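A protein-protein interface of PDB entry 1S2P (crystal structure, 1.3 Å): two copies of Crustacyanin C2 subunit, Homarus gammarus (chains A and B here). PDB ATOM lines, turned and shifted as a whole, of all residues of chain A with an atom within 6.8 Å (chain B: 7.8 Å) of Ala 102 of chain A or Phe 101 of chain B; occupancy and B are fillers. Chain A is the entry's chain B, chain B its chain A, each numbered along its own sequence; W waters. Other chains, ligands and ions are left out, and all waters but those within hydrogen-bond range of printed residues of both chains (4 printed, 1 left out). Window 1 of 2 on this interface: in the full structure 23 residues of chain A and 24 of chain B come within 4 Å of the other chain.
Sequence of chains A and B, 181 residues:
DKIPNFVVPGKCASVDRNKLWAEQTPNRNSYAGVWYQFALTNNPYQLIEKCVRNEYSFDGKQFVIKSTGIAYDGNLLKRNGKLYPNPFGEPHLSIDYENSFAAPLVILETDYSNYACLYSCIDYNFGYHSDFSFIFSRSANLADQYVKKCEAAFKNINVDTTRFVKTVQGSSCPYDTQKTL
Ser 94 of chain A touches none of the printed residues of chain B. Printed residues of chain B within 4 Å of Asp 96 of chain A: Pro 87 and Phe 88. Of the printed residues of chain B, Ala 102 of chain A touches Phe 101 and Ala 102. Printed residues of chain A within 4 Å of Pro 87 of chain B: Tyr 84 and Asp 96. Phe 101 of chain B touches just these residues of chain A: Ala 102 and Ile 122. The nearest printed residue of chain A that does not touch Glu 98 of chain B is Ile 122 of chain A (8.0 Å).
Phe 88 of chain A touches Tyr 97 of chain B, and with the chains exchanged Tyr 97 of chain A touches Phe 88 of chain B. Phe 101 of chain A touches Ile 122 of chain B, and with the chains exchanged Ile 122 of chain A touches Phe 101 of chain B. Ala 102 of chain B touches its own counterpart, Ala 102 of chain A. Ile 122 of chain A touches Ser 100 of chain B, but with the chains exchanged Ser 100 of chain A does not touch Ile 122 of chain B (5.3 Å).
O of Ala 102 of chain B sits at hydrogen-bond distance from N of Ala 102 of chain A (3.0 Å).
Water W3 lies within hydrogen-bond range of OH of Tyr 84 of chain B (2.7 Å) and OH of Tyr 84 of chain A (2.7 Å). Water W2 lies within hydrogen-bond range of O of Ser 100 of chain A and ND2 of Asn 86 of chain B. Water W4 bridges OD1 of Asp 96 of chain A and OG of Ser 94 of chain B. Water W1 lies within hydrogen-bond range of OG of Ser 94 of chain A (2.8 Å) and OD1 of Asp 96 of chain B (2.8 Å).
The backbone carbonyl oxygen (O) of Tyr 84 of chain A is in hydrogen-bond range of the backbone NH (N) of Ser 94 of chain A (2.7 Å). The side-chain carboxylate (OD1) of Asp 96 of chain B sits at hydrogen-bond distance from the side-chain hydroxyl (OH) of Tyr 84 of chain B (2.6 Å). The side-chain amide oxygen (OD1) of Asn 86 of chain B lies within hydrogen-bond range of the backbone NH (N) of Phe 88 of chain B (2.9 Å). N of Lys 82 of chain B sits at hydrogen-bond distance from O of Asp 96 of chain B (2.8 Å). The side-chain hydroxyl of Tyr 84 of chain A lies within hydrogen-bond range of the side-chain carboxylate of Asp 96 of chain A (2.6 Å). The backbone carbonyl oxygen (O) of Glu 98 of chain B sits at hydrogen-bond distance from the guanidinium group (NH2) of Arg 79 of chain B.
Among the printed residues, merely in contact across the chains: Tyr 84 of chain A with Pro 87 of chain B, Phe 88 of chain A with Lys 82 of chain B, Phe 88 of chain A with Asp 96 of chain B, Phe 88 of chain A with Tyr 97 of chain B, Phe 88 of chain A with Glu 98 of chain B, Asp 96 of chain A with Pro 87 of chain B, Asp 96 of chain A with Phe 88 of chain B, Tyr 97 of chain A with Phe 88 of chain B, Phe 101 of chain A with Ala 102 of chain B, Phe 101 of chain A with Ile 122 of chain B, Ala 102 of chain A with Phe 101 of chain B, Ile 122 of chain A with Ser 100 of chain B and Ile 122 of chain A with Phe 101 of chain B.
Hydrophobic or aromatic side chains of chain B that line the printed part of chain A: Pro 87, Phe 88, Phe 101 and Ile 122. Along chain B the printed residues that touch a printed residue of chain A span positions 82 to 122. Hydrophobic or aromatic side chains of chain A within 4 Å of the printed part of chain B: Tyr 84, Phe 88, Phe 101 and Ile 122. Among the printed residues, 14 pairs touch across the chains. Among the printed residues, no Asp or Glu carboxylate lies within 4 Å of a Lys or Arg side-chain nitrogen of the other chain.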
ATOM      1  N   TYR A  84     -19.870  17.956  16.294  1.00  0.00           N
ATOM      2  CA  TYR A  84     -19.399  18.921  15.300  1.00  0.00           C
ATOM      3  C   TYR A  84     -19.508  18.326  13.913  1.00  0.00           C
ATOM      4  O   TYR A  84     -19.610  17.126  13.773  1.00  0.00           O
ATOM      5  CB  TYR A  84     -17.950  19.347  15.582  1.00  0.00           C
ATOM      6  CG  TYR A  84     -16.964  18.219  15.857  1.00  0.00           C
ATOM      7  CD1 TYR A  84     -16.361  17.507  14.812  1.00  0.00           C
ATOM      8  CD2 TYR A  84     -16.614  17.891  17.157  1.00  0.00           C
ATOM      9  CE1 TYR A  84     -15.456  16.494  15.071  1.00  0.00           C
ATOM     10  CE2 TYR A  84     -15.712  16.877  17.431  1.00  0.00           C
ATOM     11  CZ  TYR A  84     -15.135  16.184  16.387  1.00  0.00           C
ATOM     12  OH  TYR A  84     -14.245  15.169  16.608  1.00  0.00           O
ATOM     13  N   PHE A  88     -14.644  15.799   6.898  1.00  0.00           N
ATOM     14  CA  PHE A  88     -14.483  15.665   5.451  1.00  0.00           C
ATOM     15  C   PHE A  88     -15.590  16.401   4.692  1.00  0.00           C
ATOM     16  O   PHE A  88     -15.617  16.367   3.467  1.00  0.00           O
ATOM     17  CB  PHE A  88     -14.476  14.180   5.060  1.00  0.00           C
ATOM     18  CG  PHE A  88     -13.293  13.436   5.601  1.00  0.00           C
ATOM     19  CD1 PHE A  88     -13.357  12.817   6.839  1.00  0.00           C
ATOM     20  CD2 PHE A  88     -12.102  13.391   4.897  1.00  0.00           C
ATOM     21  CE1 PHE A  88     -12.274  12.157   7.348  1.00  0.00           C
ATOM     22  CE2 PHE A  88     -11.000  12.724   5.414  1.00  0.00           C
ATOM     23  CZ  PHE A  88     -11.088  12.115   6.642  1.00  0.00           C
ATOM     24  N   SER A  94     -20.152  14.468  13.758  1.00  0.00           N
ATOM     25  CA  SER A  94     -19.333  13.534  14.507  1.00  0.00           C
ATOM     26  C   SER A  94     -19.666  13.739  15.975  1.00  0.00           C
ATOM     27  O   SER A  94     -19.654  14.873  16.436  1.00  0.00           O
ATOM     28  CB  SER A  94     -17.833  13.805  14.320  1.00  0.00           C
ATOM     29  OG  SER A  94     -17.456  13.566  12.982  1.00  0.00           O
ATOM     30  N   ILE A  95     -20.015  12.661  16.683  1.00  0.00           N
ATOM     31  CA  ILE A  95     -20.141  12.706  18.147  1.00  0.00           C
ATOM     32  C   ILE A  95     -18.794  12.201  18.723  1.00  0.00           C
ATOM     33  O   ILE A  95     -18.332  11.108  18.362  1.00  0.00           O
ATOM     34  CB  ILE A  95     -21.376  11.888  18.660  1.00  0.00           C
ATOM     35  CG1 ILE A  95     -21.469  11.883  20.190  1.00  0.00           C
ATOM     36  CG2 ILE A  95     -21.310  10.465  18.274  1.00  0.00           C
ATOM     37  CD1 ILE A  95     -21.760  13.197  20.810  1.00  0.00           C
ATOM     38  N   ASP A  96     -18.166  13.000  19.588  1.00  0.00           N
ATOM     39  CA  ASP A  96     -16.811  12.707  20.074  1.00  0.00           C
ATOM     40  C   ASP A  96     -16.810  12.788  21.594  1.00  0.00           C
ATOM     41  O   ASP A  96     -17.400  13.702  22.152  1.00  0.00           O
ATOM     42  CB  ASP A  96     -15.846  13.737  19.449  1.00  0.00           C
ATOM     43  CG  ASP A  96     -14.383  13.331  19.526  1.00  0.00           C
ATOM     44  OD1 ASP A  96     -13.553  14.045  18.884  1.00  0.00           O
ATOM     45  OD2 ASP A  96     -14.005  12.362  20.199  1.00  0.00           O
ATOM     46  N   TYR A  97     -16.192  11.839  22.287  1.00  0.00           N
ATOM     47  CA  TYR A  97     -16.100  11.937  23.733  1.00  0.00           C
ATOM     48  C   TYR A  97     -14.671  11.814  24.201  1.00  0.00           C
ATOM     49  O   TYR A  97     -13.888  11.066  23.615  1.00  0.00           O
ATOM     50  CB  TYR A  97     -16.956  10.884  24.429  1.00  0.00           C
ATOM     51  CG  TYR A  97     -18.417  11.299  24.595  1.00  0.00           C
ATOM     52  CD1 TYR A  97     -19.325  11.141  23.571  1.00  0.00           C
ATOM     53  CD2 TYR A  97     -18.859  11.908  25.753  1.00  0.00           C
ATOM     54  CE1 TYR A  97     -20.655  11.534  23.721  1.00  0.00           C
ATOM     55  CE2 TYR A  97     -20.189  12.293  25.919  1.00  0.00           C
ATOM     56  CZ  TYR A  97     -21.065  12.126  24.900  1.00  0.00           C
ATOM     57  OH  TYR A  97     -22.383  12.501  25.045  1.00  0.00           O
ATOM     58  N   SER A 100     -12.402   8.561  24.503  1.00  0.00           N
ATOM     59  CA  SER A 100     -13.095   7.640  23.628  1.00  0.00           C
ATOM     60  C   SER A 100     -12.823   8.024  22.174  1.00  0.00           C
ATOM     61  O   SER A 100     -11.922   8.811  21.846  1.00  0.00           O
ATOM     62  CB  SER A 100     -14.611   7.652  23.914  1.00  0.00           C
ATOM     63  OG  SER A 100     -15.274   6.533  23.344  1.00  0.00           O
ATOM     64  N   PHE A 101     -13.642   7.505  21.297  1.00  0.00           N
ATOM     65  CA  PHE A 101     -13.518   7.748  19.876  1.00  0.00           C
ATOM     66  C   PHE A 101     -14.663   8.627  19.395  1.00  0.00           C
ATOM     67  O   PHE A 101     -15.521   9.050  20.173  1.00  0.00           O
ATOM     68  CB  PHE A 101     -13.607   6.425  19.169  1.00  0.00           C
ATOM     69  CG  PHE A 101     -14.794   5.644  19.585  1.00  0.00           C
ATOM     70  CD1 PHE A 101     -15.994   5.773  18.934  1.00  0.00           C
ATOM     71  CD2 PHE A 101     -14.727   4.844  20.711  1.00  0.00           C
ATOM     72  CE1 PHE A 101     -17.095   5.059  19.372  1.00  0.00           C
ATOM     73  CE2 PHE A 101     -15.813   4.139  21.144  1.00  0.00           C
ATOM     74  CZ  PHE A 101     -16.991   4.244  20.481  1.00  0.00           C
ATOM     75  N   ALA A 102     -14.684   8.889  18.097  1.00  0.00           N
ATOM     76  CA  ALA A 102     -15.740   9.697  17.498  1.00  0.00           C
ATOM     77  C   ALA A 102     -16.433   8.908  16.425  1.00  0.00           C
ATOM     78  O   ALA A 102     -15.794   8.141  15.711  1.00  0.00           O
ATOM     79  CB  ALA A 102     -15.161  10.984  16.930  1.00  0.00           C
ATOM     80  N   ALA A 103     -17.750   9.083  16.306  1.00  0.00           N
ATOM     81  CA  ALA A 103     -18.569   8.333  15.366  1.00  0.00           C
ATOM     82  C   ALA A 103     -19.513   9.261  14.632  1.00  0.00           C
ATOM     83  O   ALA A 103     -19.837  10.325  15.124  1.00  0.00           O
ATOM     84  CB  ALA A 103     -19.391   7.328  16.114  1.00  0.00           C
ATOM     85  N   PRO A 104     -19.966   8.826  13.468  1.00  0.00           N
ATOM     86  CA  PRO A 104     -20.997   9.554  12.746  1.00  0.00           C
ATOM     87  C   PRO A 104     -22.289   9.464  13.560  1.00  0.00           C
ATOM     88  O   PRO A 104     -22.597   8.445  14.200  1.00  0.00           O
ATOM     89  CB  PRO A 104     -21.118   8.796  11.424  1.00  0.00           C
ATOM     90  CG  PRO A 104     -20.376   7.574  11.590  1.00  0.00           C
ATOM     91  CD  PRO A 104     -19.536   7.607  12.772  1.00  0.00           C
ATOM     92  N   ILE A 122     -21.640   1.973  11.043  1.00  0.00           N
ATOM     93  CA  ILE A 122     -20.289   1.807  10.496  1.00  0.00           C
ATOM     94  C   ILE A 122     -20.202   0.524   9.676  1.00  0.00           C
ATOM     95  O   ILE A 122     -20.676  -0.533  10.104  1.00  0.00           O
ATOM     96  CB  ILE A 122     -19.224   1.764  11.622  1.00  0.00           C
ATOM     97  CG1 ILE A 122     -17.806   1.634  11.034  1.00  0.00           C
ATOM     98  CG2 ILE A 122     -19.444   0.613  12.543  1.00  0.00           C
ATOM     99  CD1 ILE A 122     -16.925   2.818  11.257  1.00  0.00           C
ATOM    100  N   ASN B  43      -7.976  -6.250  11.973  1.00  0.00           N
ATOM    101  CA  ASN B  43      -8.633  -4.959  11.947  1.00  0.00           C
ATOM    102  C   ASN B  43      -9.869  -5.018  11.061  1.00  0.00           C
ATOM    103  O   ASN B  43      -9.747  -5.238   9.878  1.00  0.00           O
ATOM    104  CB  ASN B  43      -7.623  -3.916  11.440  1.00  0.00           C
ATOM    105  CG  ASN B  43      -8.115  -2.501  11.634  1.00  0.00           C
ATOM    106  OD1 ASN B  43      -9.270  -2.206  11.342  1.00  0.00           O
ATOM    107  ND2 ASN B  43      -7.254  -1.625  12.146  1.00  0.00           N
ATOM    108  N   PRO B  44     -11.065  -4.884  11.628  1.00  0.00           N
ATOM    109  CA  PRO B  44     -12.293  -4.953  10.838  1.00  0.00           C
ATOM    110  C   PRO B  44     -12.628  -3.686  10.069  1.00  0.00           C
ATOM    111  O   PRO B  44     -13.666  -3.614   9.394  1.00  0.00           O
ATOM    112  CB  PRO B  44     -13.381  -5.161  11.910  1.00  0.00           C
ATOM    113  CG  PRO B  44     -12.868  -4.510  13.090  1.00  0.00           C
ATOM    114  CD  PRO B  44     -11.367  -4.661  13.048  1.00  0.00           C
ATOM    115  N   TYR B  45     -11.793  -2.669  10.198  1.00  0.00           N
ATOM    116  CA  TYR B  45     -12.091  -1.354   9.624  1.00  0.00           C
ATOM    117  C   TYR B  45     -11.207  -0.990   8.439  1.00  0.00           C
ATOM    118  O   TYR B  45     -11.428   0.050   7.813  1.00  0.00           O
ATOM    119  CB  TYR B  45     -11.897  -0.265  10.678  1.00  0.00           C
ATOM    120  CG  TYR B  45     -12.660  -0.464  11.947  1.00  0.00           C
ATOM    121  CD1 TYR B  45     -12.013  -0.790  13.120  1.00  0.00           C
ATOM    122  CD2 TYR B  45     -14.034  -0.308  11.982  1.00  0.00           C
ATOM    123  CE1 TYR B  45     -12.697  -0.978  14.273  1.00  0.00           C
ATOM    124  CE2 TYR B  45     -14.732  -0.454  13.154  1.00  0.00           C
ATOM    125  CZ  TYR B  45     -14.053  -0.807  14.296  1.00  0.00           C
ATOM    126  OH  TYR B  45     -14.728  -0.988  15.488  1.00  0.00           O
ATOM    127  N   ARG B  79      -8.540   5.600  -0.239  1.00  0.00           N
ATOM    128  CA  ARG B  79      -9.285   6.050   0.947  1.00  0.00           C
ATOM    129  C   ARG B  79      -8.651   7.349   1.445  1.00  0.00           C
ATOM    130  O   ARG B  79      -7.425   7.462   1.505  1.00  0.00           O
ATOM    131  CB  ARG B  79      -9.265   5.023   2.089  1.00  0.00           C
ATOM    132  CG  ARG B  79      -9.887   3.673   1.780  1.00  0.00           C
ATOM    133  CD  ARG B  79     -11.412   3.661   1.619  1.00  0.00           C
ATOM    134  NE  ARG B  79     -12.278   3.951   2.769  1.00  0.00           N
ATOM    135  CZ  ARG B  79     -12.006   3.799   4.060  1.00  0.00           C
ATOM    136  NH1 ARG B  79     -10.831   3.374   4.496  1.00  0.00           N
ATOM    137  NH2 ARG B  79     -12.957   4.097   4.940  1.00  0.00           N
ATOM    138  N   LYS B  82      -7.401  11.677   7.609  1.00  0.00           N
ATOM    139  CA  LYS B  82      -6.838  12.830   8.303  1.00  0.00           C
ATOM    140  C   LYS B  82      -6.249  12.370   9.633  1.00  0.00           C
ATOM    141  O   LYS B  82      -6.731  11.421  10.239  1.00  0.00           O
ATOM    142  CB  LYS B  82      -7.874  13.932   8.575  1.00  0.00           C
ATOM    143  CG  LYS B  82      -8.458  14.646   7.377  1.00  0.00           C
ATOM    144  CD  LYS B  82      -9.479  15.677   7.865  1.00  0.00           C
ATOM    145  CE  LYS B  82     -10.072  16.466   6.735  1.00  0.00           C
ATOM    146  NZ  LYS B  82      -9.031  17.211   6.020  1.00  0.00           N
ATOM    147  N   TYR B  84      -5.087  14.375  13.171  1.00  0.00           N
ATOM    148  CA  TYR B  84      -5.077  15.690  13.820  1.00  0.00           C
ATOM    149  C   TYR B  84      -5.127  15.577  15.338  1.00  0.00           C
ATOM    150  O   TYR B  84      -5.533  14.544  15.870  1.00  0.00           O
ATOM    151  CB  TYR B  84      -6.251  16.542  13.338  1.00  0.00           C
ATOM    152  CG  TYR B  84      -7.603  15.846  13.341  1.00  0.00           C
ATOM    153  CD1 TYR B  84      -8.388  15.779  14.499  1.00  0.00           C
ATOM    154  CD2 TYR B  84      -8.128  15.314  12.168  1.00  0.00           C
ATOM    155  CE1 TYR B  84      -9.629  15.157  14.494  1.00  0.00           C
ATOM    156  CE2 TYR B  84      -9.367  14.698  12.155  1.00  0.00           C
ATOM    157  CZ  TYR B  84     -10.124  14.634  13.321  1.00  0.00           C
ATOM    158  OH  TYR B  84     -11.359  14.018  13.318  1.00  0.00           O
ATOM    159  N   ASN B  86      -6.162  15.380  19.117  1.00  0.00           N
ATOM    160  CA  ASN B  86      -7.423  15.054  19.734  1.00  0.00           C
ATOM    161  C   ASN B  86      -8.153  16.340  20.127  1.00  0.00           C
ATOM    162  O   ASN B  86      -7.560  17.184  20.787  1.00  0.00           O
ATOM    163  CB  ASN B  86      -7.187  14.204  20.965  1.00  0.00           C
ATOM    164  CG  ASN B  86      -8.429  14.037  21.782  1.00  0.00           C
ATOM    165  OD1 ASN B  86      -8.702  14.822  22.698  1.00  0.00           O
ATOM    166  ND2 ASN B  86      -9.222  13.040  21.429  1.00  0.00           N
ATOM    167  N   PRO B  87      -9.425  16.478  19.740  1.00  0.00           N
ATOM    168  CA  PRO B  87     -10.165  17.719  19.996  1.00  0.00           C
ATOM    169  C   PRO B  87     -10.380  18.142  21.455  1.00  0.00           C
ATOM    170  O   PRO B  87     -10.667  19.339  21.665  1.00  0.00           O
ATOM    171  CB  PRO B  87     -11.504  17.469  19.286  1.00  0.00           C
ATOM    172  CG  PRO B  87     -11.203  16.494  18.240  1.00  0.00           C
ATOM    173  CD  PRO B  87     -10.204  15.572  18.881  1.00  0.00           C
ATOM    174  N   PHE B  88     -10.234  17.239  22.422  1.00  0.00           N
ATOM    175  CA  PHE B  88     -10.349  17.604  23.837  1.00  0.00           C
ATOM    176  C   PHE B  88      -9.020  18.014  24.448  1.00  0.00           C
ATOM    177  O   PHE B  88      -8.917  18.224  25.663  1.00  0.00           O
ATOM    178  CB  PHE B  88     -10.935  16.432  24.597  1.00  0.00           C
ATOM    179  CG  PHE B  88     -12.330  16.096  24.186  1.00  0.00           C
ATOM    180  CD1 PHE B  88     -12.568  15.168  23.192  1.00  0.00           C
ATOM    181  CD2 PHE B  88     -13.403  16.721  24.768  1.00  0.00           C
ATOM    182  CE1 PHE B  88     -13.844  14.862  22.790  1.00  0.00           C
ATOM    183  CE2 PHE B  88     -14.688  16.414  24.390  1.00  0.00           C
ATOM    184  CZ  PHE B  88     -14.910  15.493  23.385  1.00  0.00           C
ATOM    185  N   SER B  94      -6.041  11.980  16.606  1.00  0.00           N
ATOM    186  CA  SER B  94      -7.210  11.280  16.122  1.00  0.00           C
ATOM    187  C   SER B  94      -6.954  10.897  14.673  1.00  0.00           C
ATOM    188  O   SER B  94      -6.555  11.775  13.886  1.00  0.00           O
ATOM    189  CB  SER B  94      -8.460  12.175  16.157  1.00  0.00           C
ATOM    190  OG  SER B  94      -8.847  12.511  17.481  1.00  0.00           O
ATOM    191  N   ILE B  95      -7.076   9.609  14.334  1.00  0.00           N
ATOM    192  CA  ILE B  95      -7.044   9.190  12.934  1.00  0.00           C
ATOM    193  C   ILE B  95      -8.488   9.032  12.464  1.00  0.00           C
ATOM    194  O   ILE B  95      -9.285   8.336  13.088  1.00  0.00           O
ATOM    195  CB  ILE B  95      -6.176   7.917  12.727  1.00  0.00           C
ATOM    196  CG1 ILE B  95      -6.056   7.567  11.245  1.00  0.00           C
ATOM    197  CG2 ILE B  95      -6.760   6.706  13.417  1.00  0.00           C
ATOM    198  CD1 ILE B  95      -4.860   8.093  10.596  1.00  0.00           C
ATOM    199  N   ASP B  96      -8.813   9.717  11.370  1.00  0.00           N
ATOM    200  CA  ASP B  96     -10.198   9.896  10.910  1.00  0.00           C
ATOM    201  C   ASP B  96     -10.234   9.587   9.436  1.00  0.00           C
ATOM    202  O   ASP B  96      -9.438  10.110   8.689  1.00  0.00           O
ATOM    203  CB  ASP B  96     -10.605  11.339  11.220  1.00  0.00           C
ATOM    204  CG  ASP B  96     -12.081  11.598  11.071  1.00  0.00           C
ATOM    205  OD1 ASP B  96     -12.533  12.715  11.455  1.00  0.00           O
ATOM    206  OD2 ASP B  96     -12.840  10.748  10.580  1.00  0.00           O
ATOM    207  N   TYR B  97     -11.104   8.670   9.027  1.00  0.00           N
ATOM    208  CA  TYR B  97     -11.213   8.297   7.623  1.00  0.00           C
ATOM    209  C   TYR B  97     -12.621   8.562   7.125  1.00  0.00           C
ATOM    210  O   TYR B  97     -13.582   8.308   7.850  1.00  0.00           O
ATOM    211  CB  TYR B  97     -10.798   6.838   7.409  1.00  0.00           C
ATOM    212  CG  TYR B  97      -9.320   6.712   7.085  1.00  0.00           C
ATOM    213  CD1 TYR B  97      -8.351   6.899   8.047  1.00  0.00           C
ATOM    214  CD2 TYR B  97      -8.911   6.421   5.812  1.00  0.00           C
ATOM    215  CE1 TYR B  97      -7.021   6.811   7.734  1.00  0.00           C
ATOM    216  CE2 TYR B  97      -7.565   6.343   5.489  1.00  0.00           C
ATOM    217  CZ  TYR B  97      -6.639   6.510   6.471  1.00  0.00           C
ATOM    218  OH  TYR B  97      -5.300   6.462   6.190  1.00  0.00           O
ATOM    219  N   GLU B  98     -12.724   9.061   5.895  1.00  0.00           N
ATOM    220  CA  GLU B  98     -14.003   9.338   5.235  1.00  0.00           C
ATOM    221  C   GLU B  98     -14.835   8.057   5.210  1.00  0.00           C
ATOM    222  O   GLU B  98     -14.299   6.976   5.002  1.00  0.00           O
ATOM    223  CB  GLU B  98     -13.725   9.808   3.813  1.00  0.00           C
ATOM    224  CG  GLU B  98     -14.872  10.484   3.090  1.00  0.00           C
ATOM    225  CD  GLU B  98     -14.435  10.999   1.732  1.00  0.00           C
ATOM    226  OE1 GLU B  98     -13.612  10.323   1.075  1.00  0.00           O
ATOM    227  OE2 GLU B  98     -14.910  12.074   1.320  1.00  0.00           O
ATOM    228  N   ASN B  99     -16.140   8.184   5.455  1.00  0.00           N
ATOM    229  CA  ASN B  99     -17.074   7.052   5.501  1.00  0.00           C
ATOM    230  C   ASN B  99     -16.699   6.036   6.566  1.00  0.00           C
ATOM    231  O   ASN B  99     -16.985   4.849   6.447  1.00  0.00           O
ATOM    232  CB  ASN B  99     -17.197   6.364   4.142  1.00  0.00           C
ATOM    233  CG  ASN B  99     -17.552   7.325   3.030  1.00  0.00           C
ATOM    234  OD1 ASN B  99     -16.852   7.390   2.025  1.00  0.00           O
ATOM    235  ND2 ASN B  99     -18.637   8.069   3.198  1.00  0.00           N
ATOM    236  N   SER B 100     -16.081   6.509   7.642  1.00  0.00           N
ATOM    237  CA  SER B 100     -15.695   5.637   8.740  1.00  0.00           C
ATOM    238  C   SER B 100     -15.733   6.463  10.030  1.00  0.00           C
ATOM    239  O   SER B 100     -16.397   7.501  10.116  1.00  0.00           O
ATOM    240  CB  SER B 100     -14.289   5.065   8.477  1.00  0.00           C
ATOM    241  OG  SER B 100     -14.006   3.960   9.311  1.00  0.00           O
ATOM    242  N   PHE B 101     -15.016   6.033  11.040  1.00  0.00           N
ATOM    243  CA  PHE B 101     -15.030   6.780  12.281  1.00  0.00           C
ATOM    244  C   PHE B 101     -13.656   7.323  12.579  1.00  0.00           C
ATOM    245  O   PHE B 101     -12.775   7.230  11.723  1.00  0.00           O
ATOM    246  CB  PHE B 101     -15.590   5.915  13.383  1.00  0.00           C
ATOM    247  CG  PHE B 101     -14.643   4.925  13.969  1.00  0.00           C
ATOM    248  CD1 PHE B 101     -14.283   3.773  13.285  1.00  0.00           C
ATOM    249  CD2 PHE B 101     -14.160   5.105  15.251  1.00  0.00           C
ATOM    250  CE1 PHE B 101     -13.427   2.844  13.871  1.00  0.00           C
ATOM    251  CE2 PHE B 101     -13.319   4.174  15.835  1.00  0.00           C
ATOM    252  CZ  PHE B 101     -12.958   3.051  15.144  1.00  0.00           C
ATOM    253  N   ALA B 102     -13.487   7.951  13.732  1.00  0.00           N
ATOM    254  CA  ALA B 102     -12.189   8.480  14.116  1.00  0.00           C
ATOM    255  C   ALA B 102     -11.759   7.843  15.428  1.00  0.00           C
ATOM    256  O   ALA B 102     -12.576   7.690  16.336  1.00  0.00           O
ATOM    257  CB  ALA B 102     -12.243   9.976  14.264  1.00  0.00           C
ATOM    258  N   ALA B 103     -10.510   7.417  15.522  1.00  0.00           N
ATOM    259  CA  ALA B 103     -10.036   6.772  16.716  1.00  0.00           C
ATOM    260  C   ALA B 103      -8.741   7.381  17.203  1.00  0.00           C
ATOM    261  O   ALA B 103      -8.027   8.017  16.447  1.00  0.00           O
ATOM    262  CB  ALA B 103      -9.797   5.330  16.423  1.00  0.00           C
ATOM    263  N   PRO B 104      -8.412   7.152  18.468  1.00  0.00           N
ATOM    264  CA  PRO B 104      -7.110   7.585  18.968  1.00  0.00           C
ATOM    265  C   PRO B 104      -5.987   6.850  18.258  1.00  0.00           C
ATOM    266  O   PRO B 104      -6.113   5.682  17.916  1.00  0.00           O
ATOM    267  CB  PRO B 104      -7.130   7.195  20.441  1.00  0.00           C
ATOM    268  CG  PRO B 104      -8.338   6.379  20.660  1.00  0.00           C
ATOM    269  CD  PRO B 104      -9.211   6.455  19.492  1.00  0.00           C
ATOM    270  N   SER B 120      -3.839   1.969  18.522  1.00  0.00           N
ATOM    271  CA  SER B 120      -5.150   2.539  18.844  1.00  0.00           C
ATOM    272  C   SER B 120      -5.887   1.608  19.804  1.00  0.00           C
ATOM    273  O   SER B 120      -5.785   0.400  19.676  1.00  0.00           O
ATOM    274  CB  SER B 120      -5.975   2.730  17.556  1.00  0.00           C
ATOM    275  OG  SER B 120      -7.236   3.333  17.804  1.00  0.00           O
ATOM    276  N   ILE B 122      -9.699   1.130  22.224  1.00  0.00           N
ATOM    277  CA  ILE B 122     -11.058   1.536  22.613  1.00  0.00           C
ATOM    278  C   ILE B 122     -11.565   0.637  23.753  1.00  0.00           C
ATOM    279  O   ILE B 122     -11.432  -0.563  23.710  1.00  0.00           O
ATOM    280  CB  ILE B 122     -12.034   1.456  21.408  1.00  0.00           C
ATOM    281  CG1 ILE B 122     -11.538   2.301  20.217  1.00  0.00           C
ATOM    282  CG2 ILE B 122     -13.450   1.837  21.844  1.00  0.00           C
ATOM    283  CD1 ILE B 122     -10.704   1.489  19.274  1.00  0.00           C
ATOM    284  N   PHE B 132      -5.831  -2.061  18.118  1.00  0.00           N
ATOM    285  CA  PHE B 132      -5.440  -2.176  16.724  1.00  0.00           C
ATOM    286  C   PHE B 132      -4.048  -1.586  16.582  1.00  0.00           C
ATOM    287  O   PHE B 132      -3.823  -0.409  16.888  1.00  0.00           O
ATOM    288  CB  PHE B 132      -6.484  -1.455  15.840  1.00  0.00           C
ATOM    289  CG  PHE B 132      -7.883  -1.930  16.125  1.00  0.00           C
ATOM    290  CD1 PHE B 132      -8.734  -1.255  16.988  1.00  0.00           C
ATOM    291  CD2 PHE B 132      -8.298  -3.127  15.608  1.00  0.00           C
ATOM    292  CE1 PHE B 132      -9.982  -1.777  17.259  1.00  0.00           C
ATOM    293  CE2 PHE B 132      -9.531  -3.656  15.933  1.00  0.00           C
ATOM    294  CZ  PHE B 132     -10.369  -2.967  16.740  1.00  0.00           C
HETATM  295  O   HOH W   1     -14.854  12.489  13.089  1.00  0.00           O
HETATM  296  O   HOH W   2      -9.668   9.999  22.808  1.00  0.00           O
HETATM  297  O   HOH W   3     -13.113  13.160  15.190  1.00  0.00           O
HETATM  298  O   HOH W   4     -11.665  12.485  17.557  1.00  0.00           O
